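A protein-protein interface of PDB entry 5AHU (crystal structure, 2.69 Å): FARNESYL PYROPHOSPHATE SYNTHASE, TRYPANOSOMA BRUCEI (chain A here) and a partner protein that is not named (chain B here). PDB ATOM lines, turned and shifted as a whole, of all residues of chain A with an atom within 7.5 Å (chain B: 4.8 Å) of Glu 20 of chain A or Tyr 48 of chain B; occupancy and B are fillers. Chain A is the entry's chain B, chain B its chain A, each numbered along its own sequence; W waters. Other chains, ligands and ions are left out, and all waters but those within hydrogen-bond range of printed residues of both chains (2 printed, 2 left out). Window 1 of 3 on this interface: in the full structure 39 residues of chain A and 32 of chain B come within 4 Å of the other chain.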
ATOM      1  N   CYS A  13     -19.975  -0.249  24.607  1.00  0.00           N
ATOM      2  CA  CYS A  13     -20.925  -0.051  23.536  1.00  0.00           C
ATOM      3  C   CYS A  13     -21.405   1.411  23.411  1.00  0.00           C
ATOM      4  O   CYS A  13     -21.423   1.984  22.316  1.00  0.00           O
ATOM      5  CB  CYS A  13     -22.109  -1.010  23.725  1.00  0.00           C
ATOM      6  SG  CYS A  13     -21.750  -2.725  23.262  1.00  0.00           S
ATOM      7  N   VAL A  14     -21.790   2.028  24.522  1.00  0.00           N
ATOM      8  CA  VAL A  14     -22.246   3.418  24.474  1.00  0.00           C
ATOM      9  C   VAL A  14     -21.106   4.297  23.960  1.00  0.00           C
ATOM     10  O   VAL A  14     -21.263   5.014  22.967  1.00  0.00           O
ATOM     11  CB  VAL A  14     -22.784   3.885  25.841  1.00  0.00           C
ATOM     12  CG1 VAL A  14     -22.984   5.403  25.887  1.00  0.00           C
ATOM     13  CG2 VAL A  14     -24.090   3.179  26.146  1.00  0.00           C
ATOM     14  N   CYS A  15     -19.948   4.195  24.600  1.00  0.00           N
ATOM     15  CA  CYS A  15     -18.744   4.906  24.150  1.00  0.00           C
ATOM     16  C   CYS A  15     -18.406   4.642  22.682  1.00  0.00           C
ATOM     17  O   CYS A  15     -17.961   5.530  21.962  1.00  0.00           O
ATOM     18  CB  CYS A  15     -17.541   4.501  24.993  1.00  0.00           C
ATOM     19  SG  CYS A  15     -17.435   5.359  26.572  1.00  0.00           S
ATOM     20  N   GLY A  16     -18.615   3.414  22.247  1.00  0.00           N
ATOM     21  CA  GLY A  16     -18.438   3.093  20.859  1.00  0.00           C
ATOM     22  C   GLY A  16     -19.332   3.893  19.962  1.00  0.00           C
ATOM     23  O   GLY A  16     -18.903   4.385  18.921  1.00  0.00           O
ATOM     24  N   TRP A  17     -20.582   4.043  20.375  1.00  0.00           N
ATOM     25  CA  TRP A  17     -21.519   4.849  19.600  1.00  0.00           C
ATOM     26  C   TRP A  17     -21.209   6.330  19.670  1.00  0.00           C
ATOM     27  O   TRP A  17     -21.302   7.011  18.655  1.00  0.00           O
ATOM     28  CB  TRP A  17     -22.960   4.574  20.003  1.00  0.00           C
ATOM     29  CG  TRP A  17     -23.423   3.315  19.409  1.00  0.00           C
ATOM     30  CD1 TRP A  17     -23.827   2.207  20.076  1.00  0.00           C
ATOM     31  CD2 TRP A  17     -23.481   2.999  18.012  1.00  0.00           C
ATOM     32  NE1 TRP A  17     -24.128   1.218  19.187  1.00  0.00           N
ATOM     33  CE2 TRP A  17     -23.929   1.671  17.911  1.00  0.00           C
ATOM     34  CE3 TRP A  17     -23.194   3.708  16.837  1.00  0.00           C
ATOM     35  CZ2 TRP A  17     -24.116   1.026  16.683  1.00  0.00           C
ATOM     36  CZ3 TRP A  17     -23.369   3.053  15.599  1.00  0.00           C
ATOM     37  CH2 TRP A  17     -23.838   1.732  15.540  1.00  0.00           C
ATOM     38  N   MET A  18     -20.823   6.832  20.839  1.00  0.00           N
ATOM     39  CA  MET A  18     -20.353   8.209  20.917  1.00  0.00           C
ATOM     40  C   MET A  18     -19.374   8.501  19.795  1.00  0.00           C
ATOM     41  O   MET A  18     -19.513   9.497  19.096  1.00  0.00           O
ATOM     42  CB  MET A  18     -19.680   8.466  22.239  1.00  0.00           C
ATOM     43  CG  MET A  18     -20.665   8.666  23.369  1.00  0.00           C
ATOM     44  SD  MET A  18     -19.850   8.813  24.962  1.00  0.00           S
ATOM     45  CE  MET A  18     -19.105  10.409  24.697  1.00  0.00           C
ATOM     46  N   ILE A  19     -18.394   7.625  19.597  1.00  0.00           N
ATOM     47  CA  ILE A  19     -17.394   7.895  18.590  1.00  0.00           C
ATOM     48  C   ILE A  19     -17.983   7.767  17.214  1.00  0.00           C
ATOM     49  O   ILE A  19     -17.664   8.570  16.326  1.00  0.00           O
ATOM     50  CB  ILE A  19     -16.192   6.964  18.669  1.00  0.00           C
ATOM     51  CG1 ILE A  19     -15.583   7.026  20.053  1.00  0.00           C
ATOM     52  CG2 ILE A  19     -15.110   7.392  17.663  1.00  0.00           C
ATOM     53  CD1 ILE A  19     -14.391   6.098  20.226  1.00  0.00           C
ATOM     54  N   GLU A  20     -18.819   6.752  17.024  1.00  0.00           N
ATOM     55  CA  GLU A  20     -19.399   6.556  15.726  1.00  0.00           C
ATOM     56  C   GLU A  20     -20.288   7.746  15.396  1.00  0.00           C
ATOM     57  O   GLU A  20     -20.328   8.187  14.245  1.00  0.00           O
ATOM     58  CB  GLU A  20     -20.181   5.241  15.654  1.00  0.00           C
ATOM     59  CG  GLU A  20     -19.353   3.959  15.600  1.00  0.00           C
ATOM     60  CD  GLU A  20     -18.436   3.840  14.388  1.00  0.00           C
ATOM     61  OE1 GLU A  20     -18.769   4.422  13.330  1.00  0.00           O
ATOM     62  OE2 GLU A  20     -17.370   3.168  14.506  1.00  0.00           O
ATOM     63  N   PHE A  21     -20.995   8.263  16.393  1.00  0.00           N
ATOM     64  CA  PHE A  21     -21.834   9.425  16.184  1.00  0.00           C
ATOM     65  C   PHE A  21     -20.988  10.658  15.970  1.00  0.00           C
ATOM     66  O   PHE A  21     -21.396  11.556  15.259  1.00  0.00           O
ATOM     67  CB  PHE A  21     -22.760   9.680  17.357  1.00  0.00           C
ATOM     68  CG  PHE A  21     -24.063   8.942  17.282  1.00  0.00           C
ATOM     69  CD1 PHE A  21     -24.085   7.578  17.221  1.00  0.00           C
ATOM     70  CD2 PHE A  21     -25.274   9.630  17.298  1.00  0.00           C
ATOM     71  CE1 PHE A  21     -25.296   6.901  17.155  1.00  0.00           C
ATOM     72  CE2 PHE A  21     -26.493   8.957  17.231  1.00  0.00           C
ATOM     73  CZ  PHE A  21     -26.511   7.591  17.160  1.00  0.00           C
ATOM     74  N   LEU A  22     -19.809  10.688  16.584  1.00  0.00           N
ATOM     75  CA  LEU A  22     -18.832  11.729  16.323  1.00  0.00           C
ATOM     76  C   LEU A  22     -18.294  11.629  14.880  1.00  0.00           C
ATOM     77  O   LEU A  22     -18.313  12.624  14.113  1.00  0.00           O
ATOM     78  CB  LEU A  22     -17.722  11.712  17.381  1.00  0.00           C
ATOM     79  CG  LEU A  22     -16.770  12.928  17.410  1.00  0.00           C
ATOM     80  CD1 LEU A  22     -17.407  14.246  17.789  1.00  0.00           C
ATOM     81  CD2 LEU A  22     -15.586  12.658  18.315  1.00  0.00           C
ATOM     82  N   GLN A  23     -17.856  10.439  14.490  1.00  0.00           N
ATOM     83  CA  GLN A  23     -17.472  10.178  13.097  1.00  0.00           C
ATOM     84  C   GLN A  23     -18.560  10.649  12.133  1.00  0.00           C
ATOM     85  O   GLN A  23     -18.293  11.333  11.143  1.00  0.00           O
ATOM     86  CB  GLN A  23     -17.156   8.695  12.951  1.00  0.00           C
ATOM     87  CG  GLN A  23     -17.044   8.096  11.567  1.00  0.00           C
ATOM     88  CD  GLN A  23     -15.911   8.692  10.789  1.00  0.00           C
ATOM     89  OE1 GLN A  23     -15.587   9.873  10.949  1.00  0.00           O
ATOM     90  NE2 GLN A  23     -15.308   7.899   9.924  1.00  0.00           N
ATOM     91  N   ALA A  24     -19.809  10.355  12.459  1.00  0.00           N
ATOM     92  CA  ALA A  24     -20.917  10.681  11.572  1.00  0.00           C
ATOM     93  C   ALA A  24     -21.076  12.182  11.397  1.00  0.00           C
ATOM     94  O   ALA A  24     -21.317  12.704  10.284  1.00  0.00           O
ATOM     95  CB  ALA A  24     -22.195  10.071  12.105  1.00  0.00           C
ATOM     96  N   HIS A  25     -20.931  12.882  12.504  1.00  0.00           N
ATOM     97  CA  HIS A  25     -20.995  14.353  12.503  1.00  0.00           C
ATOM     98  C   HIS A  25     -19.931  14.939  11.599  1.00  0.00           C
ATOM     99  O   HIS A  25     -20.218  15.786  10.785  1.00  0.00           O
ATOM    100  CB  HIS A  25     -20.830  14.868  13.929  1.00  0.00           C
ATOM    101  CG  HIS A  25     -20.226  16.223  14.014  1.00  0.00           C
ATOM    102  ND1 HIS A  25     -20.886  17.352  13.600  1.00  0.00           N
ATOM    103  CD2 HIS A  25     -19.028  16.634  14.478  1.00  0.00           C
ATOM    104  CE1 HIS A  25     -20.115  18.400  13.787  1.00  0.00           C
ATOM    105  NE2 HIS A  25     -18.979  17.990  14.309  1.00  0.00           N
ATOM    106  N   TYR A  26     -18.706  14.434  11.721  1.00  0.00           N
ATOM    107  CA  TYR A  26     -17.598  14.847  10.859  1.00  0.00           C
ATOM    108  C   TYR A  26     -17.779  14.543   9.365  1.00  0.00           C
ATOM    109  O   TYR A  26     -17.409  15.359   8.490  1.00  0.00           O
ATOM    110  CB  TYR A  26     -16.292  14.170  11.275  1.00  0.00           C
ATOM    111  CG  TYR A  26     -15.783  14.481  12.643  1.00  0.00           C
ATOM    112  CD1 TYR A  26     -16.037  15.696  13.269  1.00  0.00           C
ATOM    113  CD2 TYR A  26     -15.007  13.550  13.313  1.00  0.00           C
ATOM    114  CE1 TYR A  26     -15.570  15.943  14.558  1.00  0.00           C
ATOM    115  CE2 TYR A  26     -14.508  13.794  14.585  1.00  0.00           C
ATOM    116  CZ  TYR A  26     -14.795  14.982  15.215  1.00  0.00           C
ATOM    117  OH  TYR A  26     -14.271  15.217  16.487  1.00  0.00           O
ATOM    118  N   LEU A  27     -18.267  13.351   9.060  1.00  0.00           N
ATOM    119  CA  LEU A  27     -18.437  13.005   7.664  1.00  0.00           C
ATOM    120  C   LEU A  27     -19.505  13.879   7.024  1.00  0.00           C
ATOM    121  O   LEU A  27     -19.343  14.302   5.897  1.00  0.00           O
ATOM    122  CB  LEU A  27     -18.760  11.522   7.500  1.00  0.00           C
ATOM    123  CG  LEU A  27     -17.657  10.565   7.978  1.00  0.00           C
ATOM    124  CD1 LEU A  27     -17.984   9.163   7.511  1.00  0.00           C
ATOM    125  CD2 LEU A  27     -16.280  10.970   7.480  1.00  0.00           C
ATOM    126  N   ARG A  40     -20.231   5.661   1.450  1.00  0.00           N
ATOM    127  CA  ARG A  40     -20.682   4.304   1.791  1.00  0.00           C
ATOM    128  C   ARG A  40     -21.647   3.711   0.749  1.00  0.00           C
ATOM    129  O   ARG A  40     -22.568   2.978   1.072  1.00  0.00           O
ATOM    130  CB  ARG A  40     -21.314   4.287   3.185  1.00  0.00           C
ATOM    131  CG  ARG A  40     -20.384   4.706   4.315  1.00  0.00           C
ATOM    132  CD  ARG A  40     -21.191   4.854   5.594  1.00  0.00           C
ATOM    133  NE  ARG A  40     -20.390   5.269   6.749  1.00  0.00           N
ATOM    134  CZ  ARG A  40     -20.907   5.792   7.866  1.00  0.00           C
ATOM    135  NH1 ARG A  40     -22.220   5.956   7.987  1.00  0.00           N
ATOM    136  NH2 ARG A  40     -20.125   6.167   8.862  1.00  0.00           N
ATOM    137  N   LEU A  63     -26.021  15.505  15.412  1.00  0.00           N
ATOM    138  CA  LEU A  63     -25.164  14.332  15.582  1.00  0.00           C
ATOM    139  C   LEU A  63     -24.156  14.511  16.684  1.00  0.00           C
ATOM    140  O   LEU A  63     -23.988  13.666  17.558  1.00  0.00           O
ATOM    141  CB  LEU A  63     -24.460  13.990  14.254  1.00  0.00           C
ATOM    142  CG  LEU A  63     -25.464  13.233  13.353  1.00  0.00           C
ATOM    143  CD1 LEU A  63     -25.056  13.237  11.889  1.00  0.00           C
ATOM    144  CD2 LEU A  63     -25.702  11.793  13.879  1.00  0.00           C
ATOM    145  N   THR A  67     -24.018  12.717  20.915  1.00  0.00           N
ATOM    146  CA  THR A  67     -22.915  12.091  21.645  1.00  0.00           C
ATOM    147  C   THR A  67     -22.951  12.539  23.090  1.00  0.00           C
ATOM    148  O   THR A  67     -22.780  11.723  23.985  1.00  0.00           O
ATOM    149  CB  THR A  67     -21.513  12.442  21.077  1.00  0.00           C
ATOM    150  OG1 THR A  67     -21.242  13.841  21.238  1.00  0.00           O
ATOM    151  CG2 THR A  67     -21.404  12.093  19.603  1.00  0.00           C
ATOM    152  N   MET A  70     -26.283  11.084  24.856  1.00  0.00           N
ATOM    153  CA  MET A  70     -26.196   9.667  25.193  1.00  0.00           C
ATOM    154  C   MET A  70     -25.232   9.485  26.362  1.00  0.00           C
ATOM    155  O   MET A  70     -25.536   8.787  27.292  1.00  0.00           O
ATOM    156  CB  MET A  70     -25.880   8.791  23.959  1.00  0.00           C
ATOM    157  CG  MET A  70     -24.449   8.823  23.452  1.00  0.00           C
ATOM    158  SD  MET A  70     -24.170   7.726  22.050  1.00  0.00           S
ATOM    159  CE  MET A  70     -24.815   8.751  20.729  1.00  0.00           C
ATOM    160  N   PHE A  88     -12.896  13.453  25.451  1.00  0.00           N
ATOM    161  CA  PHE A  88     -13.672  13.399  24.252  1.00  0.00           C
ATOM    162  C   PHE A  88     -13.746  14.754  23.585  1.00  0.00           C
ATOM    163  O   PHE A  88     -13.705  14.837  22.371  1.00  0.00           O
ATOM    164  CB  PHE A  88     -15.053  12.890  24.603  1.00  0.00           C
ATOM    165  CG  PHE A  88     -15.916  12.606  23.425  1.00  0.00           C
ATOM    166  CD1 PHE A  88     -15.872  11.371  22.801  1.00  0.00           C
ATOM    167  CD2 PHE A  88     -16.805  13.551  22.980  1.00  0.00           C
ATOM    168  CE1 PHE A  88     -16.689  11.097  21.732  1.00  0.00           C
ATOM    169  CE2 PHE A  88     -17.617  13.288  21.905  1.00  0.00           C
ATOM    170  CZ  PHE A  88     -17.561  12.052  21.281  1.00  0.00           C
ATOM    171  N   TYR A 143      -8.815  10.967  16.702  1.00  0.00           N
ATOM    172  CA  TYR A 143     -10.197  10.485  16.864  1.00  0.00           C
ATOM    173  C   TYR A 143     -10.413   9.073  16.355  1.00  0.00           C
ATOM    174  O   TYR A 143     -11.340   8.388  16.771  1.00  0.00           O
ATOM    175  CB  TYR A 143     -11.203  11.432  16.251  1.00  0.00           C
ATOM    176  CG  TYR A 143     -11.667  11.139  14.848  1.00  0.00           C
ATOM    177  CD1 TYR A 143     -11.013  11.703  13.751  1.00  0.00           C
ATOM    178  CD2 TYR A 143     -12.816  10.367  14.609  1.00  0.00           C
ATOM    179  CE1 TYR A 143     -11.472  11.502  12.448  1.00  0.00           C
ATOM    180  CE2 TYR A 143     -13.282  10.145  13.310  1.00  0.00           C
ATOM    181  CZ  TYR A 143     -12.601  10.717  12.225  1.00  0.00           C
ATOM    182  OH  TYR A 143     -13.026  10.510  10.932  1.00  0.00           O
ATOM    183  N   LYS A 288      -6.937  -4.752  11.612  1.00  0.00           N
ATOM    184  CA  LYS A 288      -8.003  -4.177  10.771  1.00  0.00           C
ATOM    185  C   LYS A 288      -7.583  -3.017   9.877  1.00  0.00           C
ATOM    186  O   LYS A 288      -8.392  -2.555   9.064  1.00  0.00           O
ATOM    187  CB  LYS A 288      -9.160  -3.702  11.628  1.00  0.00           C
ATOM    188  CG  LYS A 288      -9.917  -4.843  12.271  1.00  0.00           C
ATOM    189  CD  LYS A 288     -11.048  -4.322  13.123  1.00  0.00           C
ATOM    190  CE  LYS A 288     -11.524  -5.366  14.111  1.00  0.00           C
ATOM    191  NZ  LYS A 288     -12.574  -4.780  14.989  1.00  0.00           N
ATOM    192  N   MET B   3     -20.495  -7.386  17.332  1.00  0.00           N
ATOM    193  CA  MET B   3     -21.435  -6.670  16.491  1.00  0.00           C
ATOM    194  C   MET B   3     -22.901  -6.798  16.935  1.00  0.00           C
ATOM    195  O   MET B   3     -23.673  -5.833  16.885  1.00  0.00           O
ATOM    196  CB  MET B   3     -21.307  -7.199  15.075  1.00  0.00           C
ATOM    197  CG  MET B   3     -22.040  -6.384  14.042  1.00  0.00           C
ATOM    198  SD  MET B   3     -21.195  -4.839  13.713  1.00  0.00           S
ATOM    199  CE  MET B   3     -21.891  -4.536  12.082  1.00  0.00           C
ATOM    200  N   PHE B   6     -23.620  -4.613  19.819  1.00  0.00           N
ATOM    201  CA  PHE B   6     -23.312  -3.256  19.436  1.00  0.00           C
ATOM    202  C   PHE B   6     -24.515  -2.642  18.762  1.00  0.00           C
ATOM    203  O   PHE B   6     -24.889  -1.522  19.087  1.00  0.00           O
ATOM    204  CB  PHE B   6     -22.072  -3.222  18.544  1.00  0.00           C
ATOM    205  CG  PHE B   6     -21.492  -1.844  18.353  1.00  0.00           C
ATOM    206  CD1 PHE B   6     -21.194  -1.031  19.452  1.00  0.00           C
ATOM    207  CD2 PHE B   6     -21.241  -1.355  17.074  1.00  0.00           C
ATOM    208  CE1 PHE B   6     -20.677   0.239  19.275  1.00  0.00           C
ATOM    209  CE2 PHE B   6     -20.716  -0.087  16.891  1.00  0.00           C
ATOM    210  CZ  PHE B   6     -20.432   0.712  17.994  1.00  0.00           C
ATOM    211  N   CYS B  43     -24.993   7.233  10.647  1.00  0.00           N
ATOM    212  CA  CYS B  43     -24.247   6.428  11.617  1.00  0.00           C
ATOM    213  C   CYS B  43     -24.042   4.994  11.209  1.00  0.00           C
ATOM    214  O   CYS B  43     -23.153   4.339  11.736  1.00  0.00           O
ATOM    215  CB  CYS B  43     -24.963   6.429  12.952  1.00  0.00           C
ATOM    216  SG  CYS B  43     -25.165   8.095  13.590  1.00  0.00           S
ATOM    217  N   LEU B  44     -24.903   4.493  10.325  1.00  0.00           N
ATOM    218  CA  LEU B  44     -24.858   3.085   9.938  1.00  0.00           C
ATOM    219  C   LEU B  44     -24.316   2.946   8.540  1.00  0.00           C
ATOM    220  O   LEU B  44     -24.526   3.817   7.670  1.00  0.00           O
ATOM    221  CB  LEU B  44     -26.236   2.419  10.016  1.00  0.00           C
ATOM    222  CG  LEU B  44     -26.984   2.522  11.339  1.00  0.00           C
ATOM    223  CD1 LEU B  44     -28.291   1.761  11.225  1.00  0.00           C
ATOM    224  CD2 LEU B  44     -26.150   1.975  12.482  1.00  0.00           C
ATOM    225  N   GLY B  45     -23.606   1.845   8.330  1.00  0.00           N
ATOM    226  CA  GLY B  45     -23.184   1.449   6.992  1.00  0.00           C
ATOM    227  C   GLY B  45     -21.705   1.373   6.774  1.00  0.00           C
ATOM    228  O   GLY B  45     -21.271   0.978   5.707  1.00  0.00           O
ATOM    229  N   GLY B  46     -20.919   1.796   7.759  1.00  0.00           N
ATOM    230  CA  GLY B  46     -19.463   1.653   7.687  1.00  0.00           C
ATOM    231  C   GLY B  46     -19.061   0.337   8.310  1.00  0.00           C
ATOM    232  O   GLY B  46     -19.883  -0.563   8.463  1.00  0.00           O
ATOM    233  N   LYS B  47     -17.792   0.226   8.682  1.00  0.00           N
ATOM    234  CA  LYS B  47     -17.288  -0.997   9.306  1.00  0.00           C
ATOM    235  C   LYS B  47     -17.153  -0.910  10.813  1.00  0.00           C
ATOM    236  O   LYS B  47     -16.778  -1.872  11.463  1.00  0.00           O
ATOM    237  CB  LYS B  47     -15.983  -1.437   8.621  1.00  0.00           C
ATOM    238  CG  LYS B  47     -16.188  -2.578   7.589  1.00  0.00           C
ATOM    239  CD  LYS B  47     -17.368  -2.356   6.613  1.00  0.00           C
ATOM    240  CE  LYS B  47     -17.807  -3.614   5.869  1.00  0.00           C
ATOM    241  NZ  LYS B  47     -18.840  -3.251   4.859  1.00  0.00           N
ATOM    242  N   TYR B  48     -17.504   0.239  11.366  1.00  0.00           N
ATOM    243  CA  TYR B  48     -17.630   0.429  12.793  1.00  0.00           C
ATOM    244  C   TYR B  48     -16.337   0.132  13.543  1.00  0.00           C
ATOM    245  O   TYR B  48     -16.358  -0.310  14.670  1.00  0.00           O
ATOM    246  CB  TYR B  48     -18.776  -0.426  13.337  1.00  0.00           C
ATOM    247  CG  TYR B  48     -20.064  -0.293  12.555  1.00  0.00           C
ATOM    248  CD1 TYR B  48     -20.828   0.840  12.637  1.00  0.00           C
ATOM    249  CD2 TYR B  48     -20.537  -1.329  11.773  1.00  0.00           C
ATOM    250  CE1 TYR B  48     -22.018   0.958  11.940  1.00  0.00           C
ATOM    251  CE2 TYR B  48     -21.726  -1.216  11.076  1.00  0.00           C
ATOM    252  CZ  TYR B  48     -22.459  -0.067  11.169  1.00  0.00           C
ATOM    253  OH  TYR B  48     -23.634   0.083  10.471  1.00  0.00           O
ATOM    254  N   ASN B  49     -15.202   0.387  12.924  1.00  0.00           N
ATOM    255  CA  ASN B  49     -13.923   0.096  13.576  1.00  0.00           C
ATOM    256  C   ASN B  49     -13.633   0.856  14.831  1.00  0.00           C
ATOM    257  O   ASN B  49     -12.893   0.384  15.674  1.00  0.00           O
ATOM    258  CB  ASN B  49     -12.761   0.371  12.626  1.00  0.00           C
ATOM    259  CG  ASN B  49     -12.506  -0.778  11.685  1.00  0.00           C
ATOM    260  OD1 ASN B  49     -12.757  -1.949  12.016  1.00  0.00           O
ATOM    261  ND2 ASN B  49     -12.015  -0.459  10.506  1.00  0.00           N
ATOM    262  N   ARG B  50     -14.134   2.075  14.937  1.00  0.00           N
ATOM    263  CA  ARG B  50     -13.802   2.894  16.078  1.00  0.00           C
ATOM    264  C   ARG B  50     -14.626   2.441  17.250  1.00  0.00           C
ATOM    265  O   ARG B  50     -14.106   2.220  18.338  1.00  0.00           O
ATOM    266  CB  ARG B  50     -14.043   4.339  15.764  1.00  0.00           C
ATOM    267  CG  ARG B  50     -13.149   4.858  14.647  1.00  0.00           C
ATOM    268  CD  ARG B  50     -13.538   6.295  14.361  1.00  0.00           C
ATOM    269  NE  ARG B  50     -12.747   6.915  13.309  1.00  0.00           N
ATOM    270  CZ  ARG B  50     -12.913   6.704  12.006  1.00  0.00           C
ATOM    271  NH1 ARG B  50     -13.850   5.874  11.554  1.00  0.00           N
ATOM    272  NH2 ARG B  50     -12.120   7.333  11.155  1.00  0.00           N
ATOM    273  N   GLY B  51     -15.912   2.253  17.003  1.00  0.00           N
ATOM    274  CA  GLY B  51     -16.815   1.719  17.995  1.00  0.00           C
ATOM    275  C   GLY B  51     -16.449   0.341  18.466  1.00  0.00           C
ATOM    276  O   GLY B  51     -16.457   0.092  19.649  1.00  0.00           O
ATOM    277  N   LEU B  52     -16.141  -0.555  17.541  1.00  0.00           N
ATOM    278  CA  LEU B  52     -15.866  -1.950  17.858  1.00  0.00           C
ATOM    279  C   LEU B  52     -14.554  -2.118  18.631  1.00  0.00           C
ATOM    280  O   LEU B  52     -14.439  -2.983  19.510  1.00  0.00           O
ATOM    281  CB  LEU B  52     -15.878  -2.797  16.587  1.00  0.00           C
ATOM    282  CG  LEU B  52     -17.283  -3.094  15.981  1.00  0.00           C
ATOM    283  CD1 LEU B  52     -17.204  -3.741  14.595  1.00  0.00           C
ATOM    284  CD2 LEU B  52     -18.187  -3.951  16.871  1.00  0.00           C
ATOM    285  N   THR B  53     -13.591  -1.257  18.322  1.00  0.00           N
ATOM    286  CA  THR B  53     -12.347  -1.167  19.057  1.00  0.00           C
ATOM    287  C   THR B  53     -12.561  -0.857  20.528  1.00  0.00           C
ATOM    288  O   THR B  53     -11.882  -1.401  21.369  1.00  0.00           O
ATOM    289  CB  THR B  53     -11.461  -0.071  18.482  1.00  0.00           C
ATOM    290  OG1 THR B  53     -11.202  -0.314  17.094  1.00  0.00           O
ATOM    291  CG2 THR B  53     -10.164  -0.011  19.222  1.00  0.00           C
HETATM  292  O   HOH W   1     -15.381   3.661  13.117  1.00  0.00           O
HETATM  293  O   HOH W   2      -9.735  -3.033  15.509  1.00  0.00           O
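Hydrophobic or aromatic side chains of chain B within 4 Å of the printed part of chain A: Phe 6 and Leu 44.
Printed residues of chain A that touch a printed residue of chain B: Cys 13, Gly 16, Trp 17, Ile 19, Glu 20, Phe 21, Gln 23, Ala 24, Arg 40, Leu 63, Tyr 143 and Lys 288.
Hydrophobic or aromatic side chains of chain A that line the printed part of chain B: Trp 17, Ile 19, Phe 21, Ala 24, Leu 63 and Tyr 143.
Among the printed residues, 20 pairs touch across the chains.
The backbone NH (N) of Gly 45 of chain B sits at hydrogen-bond distance from the side-chain hydroxyl (OH) of Tyr 48 of chain B (2.8 Å).
OH of Tyr 143 of chain A sits at hydrogen-bond distance from OE1 of Gln 23 of chain A, at 2.6 Å.
The backbone carbonyl oxygen of Phe 6 of chain B lies within hydrogen-bond range of the indole nitrogen of Trp 17 of chain A (2.8 Å).
The backbone carbonyl oxygen (O) of Leu 44 of chain B lies within hydrogen-bond range of the guanidinium group (NH1) of Arg 40 of chain A (3.2 Å).
The side-chain carboxylate of Glu 20 of chain A is in hydrogen-bond range of the backbone NH of Arg 50 of chain B (3.4 Å).
The side-chain amide nitrogen of Gln 23 of chain A lies close to the guanidinium group of Arg 50 of chain B.
NH2 of Arg 50 of chain B lies within hydrogen-bond range of OH of Tyr 143 of chain A, 3.3 Å away.
The backbone NH (N) of Gly 51 of chain B sits at hydrogen-bond distance from the side-chain carboxylate (OE2) of Glu 20 of chain A (3.0 Å).
Among the printed residues, pairs that only touch across the chains: Lys 288 of chain A with Asn 49 of chain B (3.1 Å), Glu 20 of chain A with Tyr 48 of chain B (3.2 Å), Gly 16 of chain A with Gly 51 of chain B (3.5 Å), Cys 13 of chain A with Phe 6 of chain B (3.6 Å), Arg 40 of chain A with Gly 46 of chain B (3.7 Å), Arg 40 of chain A with Gly 45 of chain B (3.7 Å), Leu 63 of chain A with Cys 43 of chain B (3.7 Å), Ile 19 of chain A with Arg 50 of chain B (3.8 Å), Phe 21 of chain A with Cys 43 of chain B (3.8 Å), Arg 40 of chain A with Cys 43 of chain B (3.8 Å), Trp 17 of chain A with Leu 44 of chain B (3.8 Å), Ala 24 of chain A with Cys 43 of chain B (3.9 Å), Glu 20 of chain A with Asn 49 of chain B (3.9 Å) and Gly 16 of chain A with Phe 6 of chain B (3.9 Å).
Water W1 lies within hydrogen-bond range of the side-chain carboxylate of Glu 20 of chain A (2.5 Å), the backbone NH of Arg 50 of chain B (2.7 Å) and the backbone NH of Asn 49 of chain B (3.3 Å).
Water W2 lies within hydrogen-bond range of the side-chain amino group of Lys 288 of chain A (3.4 Å) and the side-chain hydroxyl of Thr 53 of chain B (3.5 Å).
Tyr 48 of chain B touches just one residue of chain A: Glu 20 (3.2 Å).
Printed residues of chain A within 4 Å of Gly 51 of chain B: Gly 16 and Glu 20.
Printed residues of chain B within 4 Å of Cys 13 of chain A: Phe 6 (3.6 Å).
Of the printed residues of chain B, Tyr 143 of chain A touches Arg 50 (3.3 Å).
Printed residues of chain A within 4 Å of Cys 43 of chain B: Phe 21 (3.8 Å), Ala 24 (3.9 Å), Arg 40 (3.8 Å) and Leu 63 (3.7 Å).
Of the printed residues of chain B, Leu 63 of chain A touches Cys 43.
Met 70 of chain A touches none of the printed residues of chain B.
Val 14 of chain A touches none of the printed residues of chain B.
The nearest printed residue of chain A that does not touch Arg 50 of chain B is Gly 16 of chain A (5.0 Å).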
